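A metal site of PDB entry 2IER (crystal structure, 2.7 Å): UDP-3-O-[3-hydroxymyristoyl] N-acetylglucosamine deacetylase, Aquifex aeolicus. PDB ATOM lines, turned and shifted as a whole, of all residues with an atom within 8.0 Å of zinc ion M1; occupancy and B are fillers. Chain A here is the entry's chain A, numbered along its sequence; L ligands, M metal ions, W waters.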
ATOM      1  N   ILE A  18      29.603 -21.461  14.147  1.00  0.00           N
ATOM      2  CA  ILE A  18      28.155 -21.454  13.943  1.00  0.00           C
ATOM      3  C   ILE A  18      27.484 -20.131  14.353  1.00  0.00           C
ATOM      4  O   ILE A  18      26.538 -19.696  13.712  1.00  0.00           O
ATOM      5  CB  ILE A  18      27.467 -22.644  14.692  1.00  0.00           C
ATOM      6  CG1 ILE A  18      26.071 -22.865  14.098  1.00  0.00           C
ATOM      7  CG2 ILE A  18      27.365 -22.347  16.195  1.00  0.00           C
ATOM      8  CD1 ILE A  18      25.306 -24.015  14.715  1.00  0.00           C
ATOM      9  N   HIS A  58      22.814 -20.950  24.111  1.00  0.00           N
ATOM     10  CA  HIS A  58      23.030 -21.488  22.763  1.00  0.00           C
ATOM     11  C   HIS A  58      24.457 -21.970  22.472  1.00  0.00           C
ATOM     12  O   HIS A  58      24.785 -22.330  21.352  1.00  0.00           O
ATOM     13  CB  HIS A  58      22.579 -20.454  21.723  1.00  0.00           C
ATOM     14  CG  HIS A  58      21.197 -19.925  21.956  1.00  0.00           C
ATOM     15  ND1 HIS A  58      20.089 -20.743  22.047  1.00  0.00           N
ATOM     16  CD2 HIS A  58      20.741 -18.659  22.167  1.00  0.00           C
ATOM     17  CE1 HIS A  58      19.011 -20.011  22.291  1.00  0.00           C
ATOM     18  NE2 HIS A  58      19.386 -18.739  22.374  1.00  0.00           N
ATOM     19  N   SER A  59      25.291 -21.972  23.509  1.00  0.00           N
ATOM     20  CA  SER A  59      26.666 -22.439  23.431  1.00  0.00           C
ATOM     21  C   SER A  59      27.352 -22.138  24.751  1.00  0.00           C
ATOM     22  O   SER A  59      26.826 -21.382  25.568  1.00  0.00           O
ATOM     23  CB  SER A  59      27.432 -21.753  22.273  1.00  0.00           C
ATOM     24  OG  SER A  59      27.718 -20.402  22.540  1.00  0.00           O
ATOM     25  N   THR A  60      28.506 -22.752  24.978  1.00  0.00           N
ATOM     26  CA  THR A  60      29.248 -22.495  26.209  1.00  0.00           C
ATOM     27  C   THR A  60      30.491 -21.698  25.824  1.00  0.00           C
ATOM     28  O   THR A  60      31.331 -22.159  25.051  1.00  0.00           O
ATOM     29  CB  THR A  60      29.674 -23.787  26.908  1.00  0.00           C
ATOM     30  OG1 THR A  60      28.522 -24.579  27.194  1.00  0.00           O
ATOM     31  CG2 THR A  60      30.409 -23.475  28.207  1.00  0.00           C
ATOM     32  N   THR A  71      31.590 -21.345  21.994  1.00  0.00           N
ATOM     33  CA  THR A  71      31.295 -22.715  21.612  1.00  0.00           C
ATOM     34  C   THR A  71      32.408 -23.730  21.829  1.00  0.00           C
ATOM     35  O   THR A  71      32.901 -24.343  20.866  1.00  0.00           O
ATOM     36  CB  THR A  71      30.860 -22.758  20.134  1.00  0.00           C
ATOM     37  OG1 THR A  71      30.054 -21.599  19.850  1.00  0.00           O
ATOM     38  CG2 THR A  71      30.035 -23.999  19.842  1.00  0.00           C
ATOM     39  N   GLU A  73      32.004 -26.425  23.827  1.00  0.00           N
ATOM     40  CA  GLU A  73      31.396 -27.691  24.210  1.00  0.00           C
ATOM     41  C   GLU A  73      31.726 -28.933  23.399  1.00  0.00           C
ATOM     42  O   GLU A  73      31.907 -30.000  23.967  1.00  0.00           O
ATOM     43  CB  GLU A  73      29.875 -27.554  24.276  1.00  0.00           C
ATOM     44  CG  GLU A  73      29.234 -27.048  22.986  1.00  0.00           C
ATOM     45  CD  GLU A  73      29.018 -25.549  23.008  1.00  0.00           C
ATOM     46  OE1 GLU A  73      29.909 -24.819  23.466  1.00  0.00           O
ATOM     47  OE2 GLU A  73      27.942 -25.097  22.558  1.00  0.00           O
ATOM     48  N   HIS A  74      31.821 -28.811  22.085  1.00  0.00           N
ATOM     49  CA  HIS A  74      32.098 -29.986  21.271  1.00  0.00           C
ATOM     50  C   HIS A  74      33.547 -30.458  21.333  1.00  0.00           C
ATOM     51  O   HIS A  74      33.814 -31.663  21.425  1.00  0.00           O
ATOM     52  CB  HIS A  74      31.684 -29.730  19.821  1.00  0.00           C
ATOM     53  CG  HIS A  74      30.226 -29.396  19.677  1.00  0.00           C
ATOM     54  ND1 HIS A  74      29.679 -28.929  18.501  1.00  0.00           N
ATOM     55  CD2 HIS A  74      29.199 -29.460  20.562  1.00  0.00           C
ATOM     56  CE1 HIS A  74      28.383 -28.706  18.677  1.00  0.00           C
ATOM     57  NE2 HIS A  74      28.075 -29.030  19.920  1.00  0.00           N
ATOM     58  N   ILE A  98      32.568 -24.903  13.941  1.00  0.00           N
ATOM     59  CA  ILE A  98      31.468 -25.838  14.185  1.00  0.00           C
ATOM     60  C   ILE A  98      31.564 -27.117  13.371  1.00  0.00           C
ATOM     61  O   ILE A  98      30.999 -28.144  13.747  1.00  0.00           O
ATOM     62  CB  ILE A  98      30.102 -25.154  13.899  1.00  0.00           C
ATOM     63  CG1 ILE A  98      28.968 -26.024  14.444  1.00  0.00           C
ATOM     64  CG2 ILE A  98      29.928 -24.961  12.406  1.00  0.00           C
ATOM     65  CD1 ILE A  98      28.912 -26.074  15.964  1.00  0.00           C
ATOM     66  N   GLY A 101      28.845 -29.890  12.753  1.00  0.00           N
ATOM     67  CA  GLY A 101      27.895 -29.761  13.847  1.00  0.00           C
ATOM     68  C   GLY A 101      28.020 -30.787  14.948  1.00  0.00           C
ATOM     69  O   GLY A 101      27.369 -30.661  15.988  1.00  0.00           O
ATOM     70  N   SER A 102      28.859 -31.799  14.745  1.00  0.00           N
ATOM     71  CA  SER A 102      29.069 -32.855  15.743  1.00  0.00           C
ATOM     72  C   SER A 102      30.533 -32.850  16.187  1.00  0.00           C
ATOM     73  O   SER A 102      31.247 -31.875  15.996  1.00  0.00           O
ATOM     74  CB  SER A 102      28.715 -34.231  15.154  1.00  0.00           C
ATOM     75  OG  SER A 102      29.740 -34.715  14.301  1.00  0.00           O
ATOM     76  N   ALA A 177      26.279 -37.230  16.467  1.00  0.00           N
ATOM     77  CA  ALA A 177      25.010 -36.512  16.616  1.00  0.00           C
ATOM     78  C   ALA A 177      25.247 -34.995  16.480  1.00  0.00           C
ATOM     79  O   ALA A 177      26.053 -34.405  17.199  1.00  0.00           O
ATOM     80  CB  ALA A 177      24.396 -36.845  17.978  1.00  0.00           C
ATOM     81  N   ARG A 178      24.528 -34.369  15.535  1.00  0.00           N
ATOM     82  CA  ARG A 178      24.680 -32.950  15.277  1.00  0.00           C
ATOM     83  C   ARG A 178      23.820 -32.020  16.105  1.00  0.00           C
ATOM     84  O   ARG A 178      22.847 -32.427  16.732  1.00  0.00           O
ATOM     85  CB  ARG A 178      24.407 -32.678  13.800  1.00  0.00           C
ATOM     86  CG  ARG A 178      25.373 -33.338  12.851  1.00  0.00           C
ATOM     87  CD  ARG A 178      24.850 -33.305  11.434  1.00  0.00           C
ATOM     88  NE  ARG A 178      23.632 -34.098  11.308  1.00  0.00           N
ATOM     89  CZ  ARG A 178      22.887 -34.172  10.210  1.00  0.00           C
ATOM     90  NH1 ARG A 178      23.233 -33.499   9.128  1.00  0.00           N
ATOM     91  NH2 ARG A 178      21.796 -34.928  10.200  1.00  0.00           N
ATOM     92  N   THR A 179      24.198 -30.734  16.101  1.00  0.00           N
ATOM     93  CA  THR A 179      23.460 -29.699  16.810  1.00  0.00           C
ATOM     94  C   THR A 179      22.196 -29.512  15.989  1.00  0.00           C
ATOM     95  O   THR A 179      22.217 -29.610  14.764  1.00  0.00           O
ATOM     96  CB  THR A 179      24.217 -28.358  16.837  1.00  0.00           C
ATOM     97  OG1 THR A 179      24.031 -27.670  15.600  1.00  0.00           O
ATOM     98  CG2 THR A 179      25.689 -28.586  17.021  1.00  0.00           C
ATOM     99  N   PHE A 180      21.104 -29.214  16.674  1.00  0.00           N
ATOM    100  CA  PHE A 180      19.811 -29.052  16.011  1.00  0.00           C
ATOM    101  C   PHE A 180      19.138 -27.756  16.433  1.00  0.00           C
ATOM    102  O   PHE A 180      19.458 -27.173  17.472  1.00  0.00           O
ATOM    103  CB  PHE A 180      18.915 -30.228  16.394  1.00  0.00           C
ATOM    104  CG  PHE A 180      18.692 -30.346  17.871  1.00  0.00           C
ATOM    105  CD1 PHE A 180      17.548 -29.826  18.459  1.00  0.00           C
ATOM    106  CD2 PHE A 180      19.644 -30.952  18.691  1.00  0.00           C
ATOM    107  CE1 PHE A 180      17.341 -29.910  19.847  1.00  0.00           C
ATOM    108  CE2 PHE A 180      19.456 -31.047  20.079  1.00  0.00           C
ATOM    109  CZ  PHE A 180      18.300 -30.521  20.655  1.00  0.00           C
ATOM    110  N   HIS A 226      22.794 -35.666  20.978  1.00  0.00           N
ATOM    111  CA  HIS A 226      23.627 -34.472  20.935  1.00  0.00           C
ATOM    112  C   HIS A 226      23.642 -33.801  22.301  1.00  0.00           C
ATOM    113  O   HIS A 226      24.680 -33.324  22.750  1.00  0.00           O
ATOM    114  CB  HIS A 226      23.130 -33.467  19.899  1.00  0.00           C
ATOM    115  CG  HIS A 226      24.034 -32.300  19.733  1.00  0.00           C
ATOM    116  ND1 HIS A 226      25.234 -32.378  19.054  1.00  0.00           N
ATOM    117  CD2 HIS A 226      23.982 -31.046  20.261  1.00  0.00           C
ATOM    118  CE1 HIS A 226      25.879 -31.225  19.166  1.00  0.00           C
ATOM    119  NE2 HIS A 226      25.144 -30.404  19.892  1.00  0.00           N
ATOM    120  N   LYS A 227      22.481 -33.778  22.960  1.00  0.00           N
ATOM    121  CA  LYS A 227      22.403 -33.179  24.283  1.00  0.00           C
ATOM    122  C   LYS A 227      23.342 -33.924  25.227  1.00  0.00           C
ATOM    123  O   LYS A 227      24.011 -33.328  26.064  1.00  0.00           O
ATOM    124  CB  LYS A 227      20.971 -33.238  24.811  1.00  0.00           C
ATOM    125  CG  LYS A 227      20.056 -32.243  24.167  1.00  0.00           C
ATOM    126  CD  LYS A 227      20.546 -30.828  24.424  1.00  0.00           C
ATOM    127  CE  LYS A 227      19.405 -29.852  24.335  1.00  0.00           C
ATOM    128  NZ  LYS A 227      19.738 -28.596  25.042  1.00  0.00           N
ATOM    129  N   PHE A 229      25.952 -35.482  24.293  1.00  0.00           N
ATOM    130  CA  PHE A 229      27.260 -35.033  23.831  1.00  0.00           C
ATOM    131  C   PHE A 229      27.629 -33.669  24.444  1.00  0.00           C
ATOM    132  O   PHE A 229      28.727 -33.482  24.939  1.00  0.00           O
ATOM    133  CB  PHE A 229      27.261 -34.939  22.307  1.00  0.00           C
ATOM    134  CG  PHE A 229      28.553 -34.463  21.712  1.00  0.00           C
ATOM    135  CD1 PHE A 229      29.708 -35.257  21.792  1.00  0.00           C
ATOM    136  CD2 PHE A 229      28.618 -33.246  21.036  1.00  0.00           C
ATOM    137  CE1 PHE A 229      30.900 -34.838  21.208  1.00  0.00           C
ATOM    138  CE2 PHE A 229      29.820 -32.820  20.445  1.00  0.00           C
ATOM    139  CZ  PHE A 229      30.964 -33.616  20.519  1.00  0.00           C
ATOM    140  N   ASP A 230      26.694 -32.720  24.408  1.00  0.00           N
ATOM    141  CA  ASP A 230      26.922 -31.383  24.973  1.00  0.00           C
ATOM    142  C   ASP A 230      27.232 -31.438  26.465  1.00  0.00           C
ATOM    143  O   ASP A 230      28.130 -30.764  26.947  1.00  0.00           O
ATOM    144  CB  ASP A 230      25.698 -30.478  24.794  1.00  0.00           C
ATOM    145  CG  ASP A 230      25.618 -29.853  23.429  1.00  0.00           C
ATOM    146  OD1 ASP A 230      26.678 -29.676  22.789  1.00  0.00           O
ATOM    147  OD2 ASP A 230      24.488 -29.520  23.003  1.00  0.00           O
ATOM    148  N   LEU A 231      26.461 -32.240  27.188  1.00  0.00           N
ATOM    149  CA  LEU A 231      26.633 -32.369  28.630  1.00  0.00           C
ATOM    150  C   LEU A 231      28.001 -32.950  28.994  1.00  0.00           C
ATOM    151  O   LEU A 231      28.594 -32.553  29.990  1.00  0.00           O
ATOM    152  CB  LEU A 231      25.503 -33.208  29.217  1.00  0.00           C
ATOM    153  CG  LEU A 231      25.530 -33.501  30.720  1.00  0.00           C
ATOM    154  CD1 LEU A 231      25.864 -32.238  31.515  1.00  0.00           C
ATOM    155  CD2 LEU A 231      24.192 -34.081  31.137  1.00  0.00           C
ATOM    156  N   ASP A 234      30.374 -30.093  28.790  1.00  0.00           N
ATOM    157  CA  ASP A 234      30.209 -29.156  29.883  1.00  0.00           C
ATOM    158  C   ASP A 234      30.760 -29.739  31.190  1.00  0.00           C
ATOM    159  O   ASP A 234      31.310 -29.011  32.014  1.00  0.00           O
ATOM    160  CB  ASP A 234      28.729 -28.783  30.058  1.00  0.00           C
ATOM    161  CG  ASP A 234      28.229 -27.840  28.959  1.00  0.00           C
ATOM    162  OD1 ASP A 234      29.056 -27.103  28.386  1.00  0.00           O
ATOM    163  OD2 ASP A 234      27.002 -27.824  28.673  1.00  0.00           O
ATOM    164  N   HIS A 253      22.987 -25.972  28.246  1.00  0.00           N
ATOM    165  CA  HIS A 253      24.316 -25.545  28.732  1.00  0.00           C
ATOM    166  C   HIS A 253      24.241 -24.756  30.037  1.00  0.00           C
ATOM    167  O   HIS A 253      25.082 -24.902  30.931  1.00  0.00           O
ATOM    168  CB  HIS A 253      24.989 -24.674  27.677  1.00  0.00           C
ATOM    169  CG  HIS A 253      25.300 -25.391  26.405  1.00  0.00           C
ATOM    170  ND1 HIS A 253      26.087 -26.515  26.360  1.00  0.00           N
ATOM    171  CD2 HIS A 253      24.915 -25.141  25.132  1.00  0.00           C
ATOM    172  CE1 HIS A 253      26.178 -26.927  25.107  1.00  0.00           C
ATOM    173  NE2 HIS A 253      25.479 -26.108  24.342  1.00  0.00           N
HETATM  174  N1  LIG L   1      14.263 -28.540  24.049  1.00  0.00           N
HETATM  175  C1  LIG L   1      12.965 -29.089  24.132  1.00  0.00           C
HETATM  176  N2  LIG L   1      12.736 -30.125  25.015  1.00  0.00           N
HETATM  177  C2  LIG L   1      13.747 -30.663  25.820  1.00  0.00           C
HETATM  178  C3  LIG L   1      15.044 -30.123  25.741  1.00  0.00           C
HETATM  179  C4  LIG L   1      15.296 -29.058  24.850  1.00  0.00           C
HETATM  180  O1  LIG L   1      11.995 -28.691  23.458  1.00  0.00           O
HETATM  181  O2  LIG L   1      13.431 -31.598  26.580  1.00  0.00           O
HETATM  182  C5  LIG L   1      14.532 -27.414  23.102  1.00  0.00           C
HETATM  183  C6  LIG L   1      14.558 -26.006  23.730  1.00  0.00           C
HETATM  184  O3  LIG L   1      13.258 -25.508  24.022  1.00  0.00           O
HETATM  185  C7  LIG L   1      15.386 -25.240  22.699  1.00  0.00           C
HETATM  186  C8  LIG L   1      16.215 -26.337  21.888  1.00  0.00           C
HETATM  187  O4  LIG L   1      15.801 -27.576  22.463  1.00  0.00           O
HETATM  188  O5  LIG L   1      14.629 -24.747  21.632  1.00  0.00           O
HETATM  189  C9  LIG L   1      17.694 -26.039  22.252  1.00  0.00           C
HETATM  190  O6  LIG L   1      17.859 -24.919  23.128  1.00  0.00           O
HETATM  191  P1  LIG L   1      18.139 -25.048  24.720  1.00  0.00           P
HETATM  192  O7  LIG L   1      18.131 -26.469  25.107  1.00  0.00           O
HETATM  193  O8  LIG L   1      17.107 -24.244  25.429  1.00  0.00           O
HETATM  194  O9  LIG L   1      19.634 -24.520  24.963  1.00  0.00           O
HETATM  195  P2  LIG L   1      21.142 -24.963  24.549  1.00  0.00           P
HETATM  196  O10 LIG L   1      21.968 -24.061  25.416  1.00  0.00           O
HETATM  197  O11 LIG L   1      21.270 -24.626  23.104  1.00  0.00           O
HETATM  198  O12 LIG L   1      21.410 -26.388  24.878  1.00  0.00           O
HETATM  199 ZN    ZN M   1      26.128 -28.818  20.867  1.00  0.00          ZN
HETATM  200 ZN    ZN M   2      25.687 -25.965  21.947  1.00  0.00          ZN
HETATM  201  O   HOH W   1      25.194 -26.773  19.820  1.00  0.00           O
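The side-chain amino group (NZ) of Lys 227 is in salt-bridge range of an oxygen (O7) of the ligand (2.7 Å). The backbone NH (N) of His 58 sits at hydrogen-bond distance from an oxygen (O10) of the ligand (3.5 Å).
ND1 of His 226 sits close to O of Arg 178, at 3.3 Å. A ring nitrogen (ND1) of His 226 lies within hydrogen-bond range of the backbone carbonyl oxygen (O) of Ala 177, at 2.9 Å. The backbone carbonyl oxygen (O) of Gly 101 lies close to the backbone NH (N) of Thr 179, at 3.2 Å.
Thr 179 touches zinc ion M1. Within 4 Å of zinc ion M1: His 74, Thr 179, His 226 and Asp 230.
Zinc ion M1 is bound by a ring nitrogen (NE2) of His 226, a ring nitrogen (NE2) of His 74, the side-chain carboxylate of Asp 230 and water W1. Zinc ion M1 has four donor atoms within binding distance. Slightly farther from zinc ion M1 lies OD2 of Asp 230 (2.8 Å).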
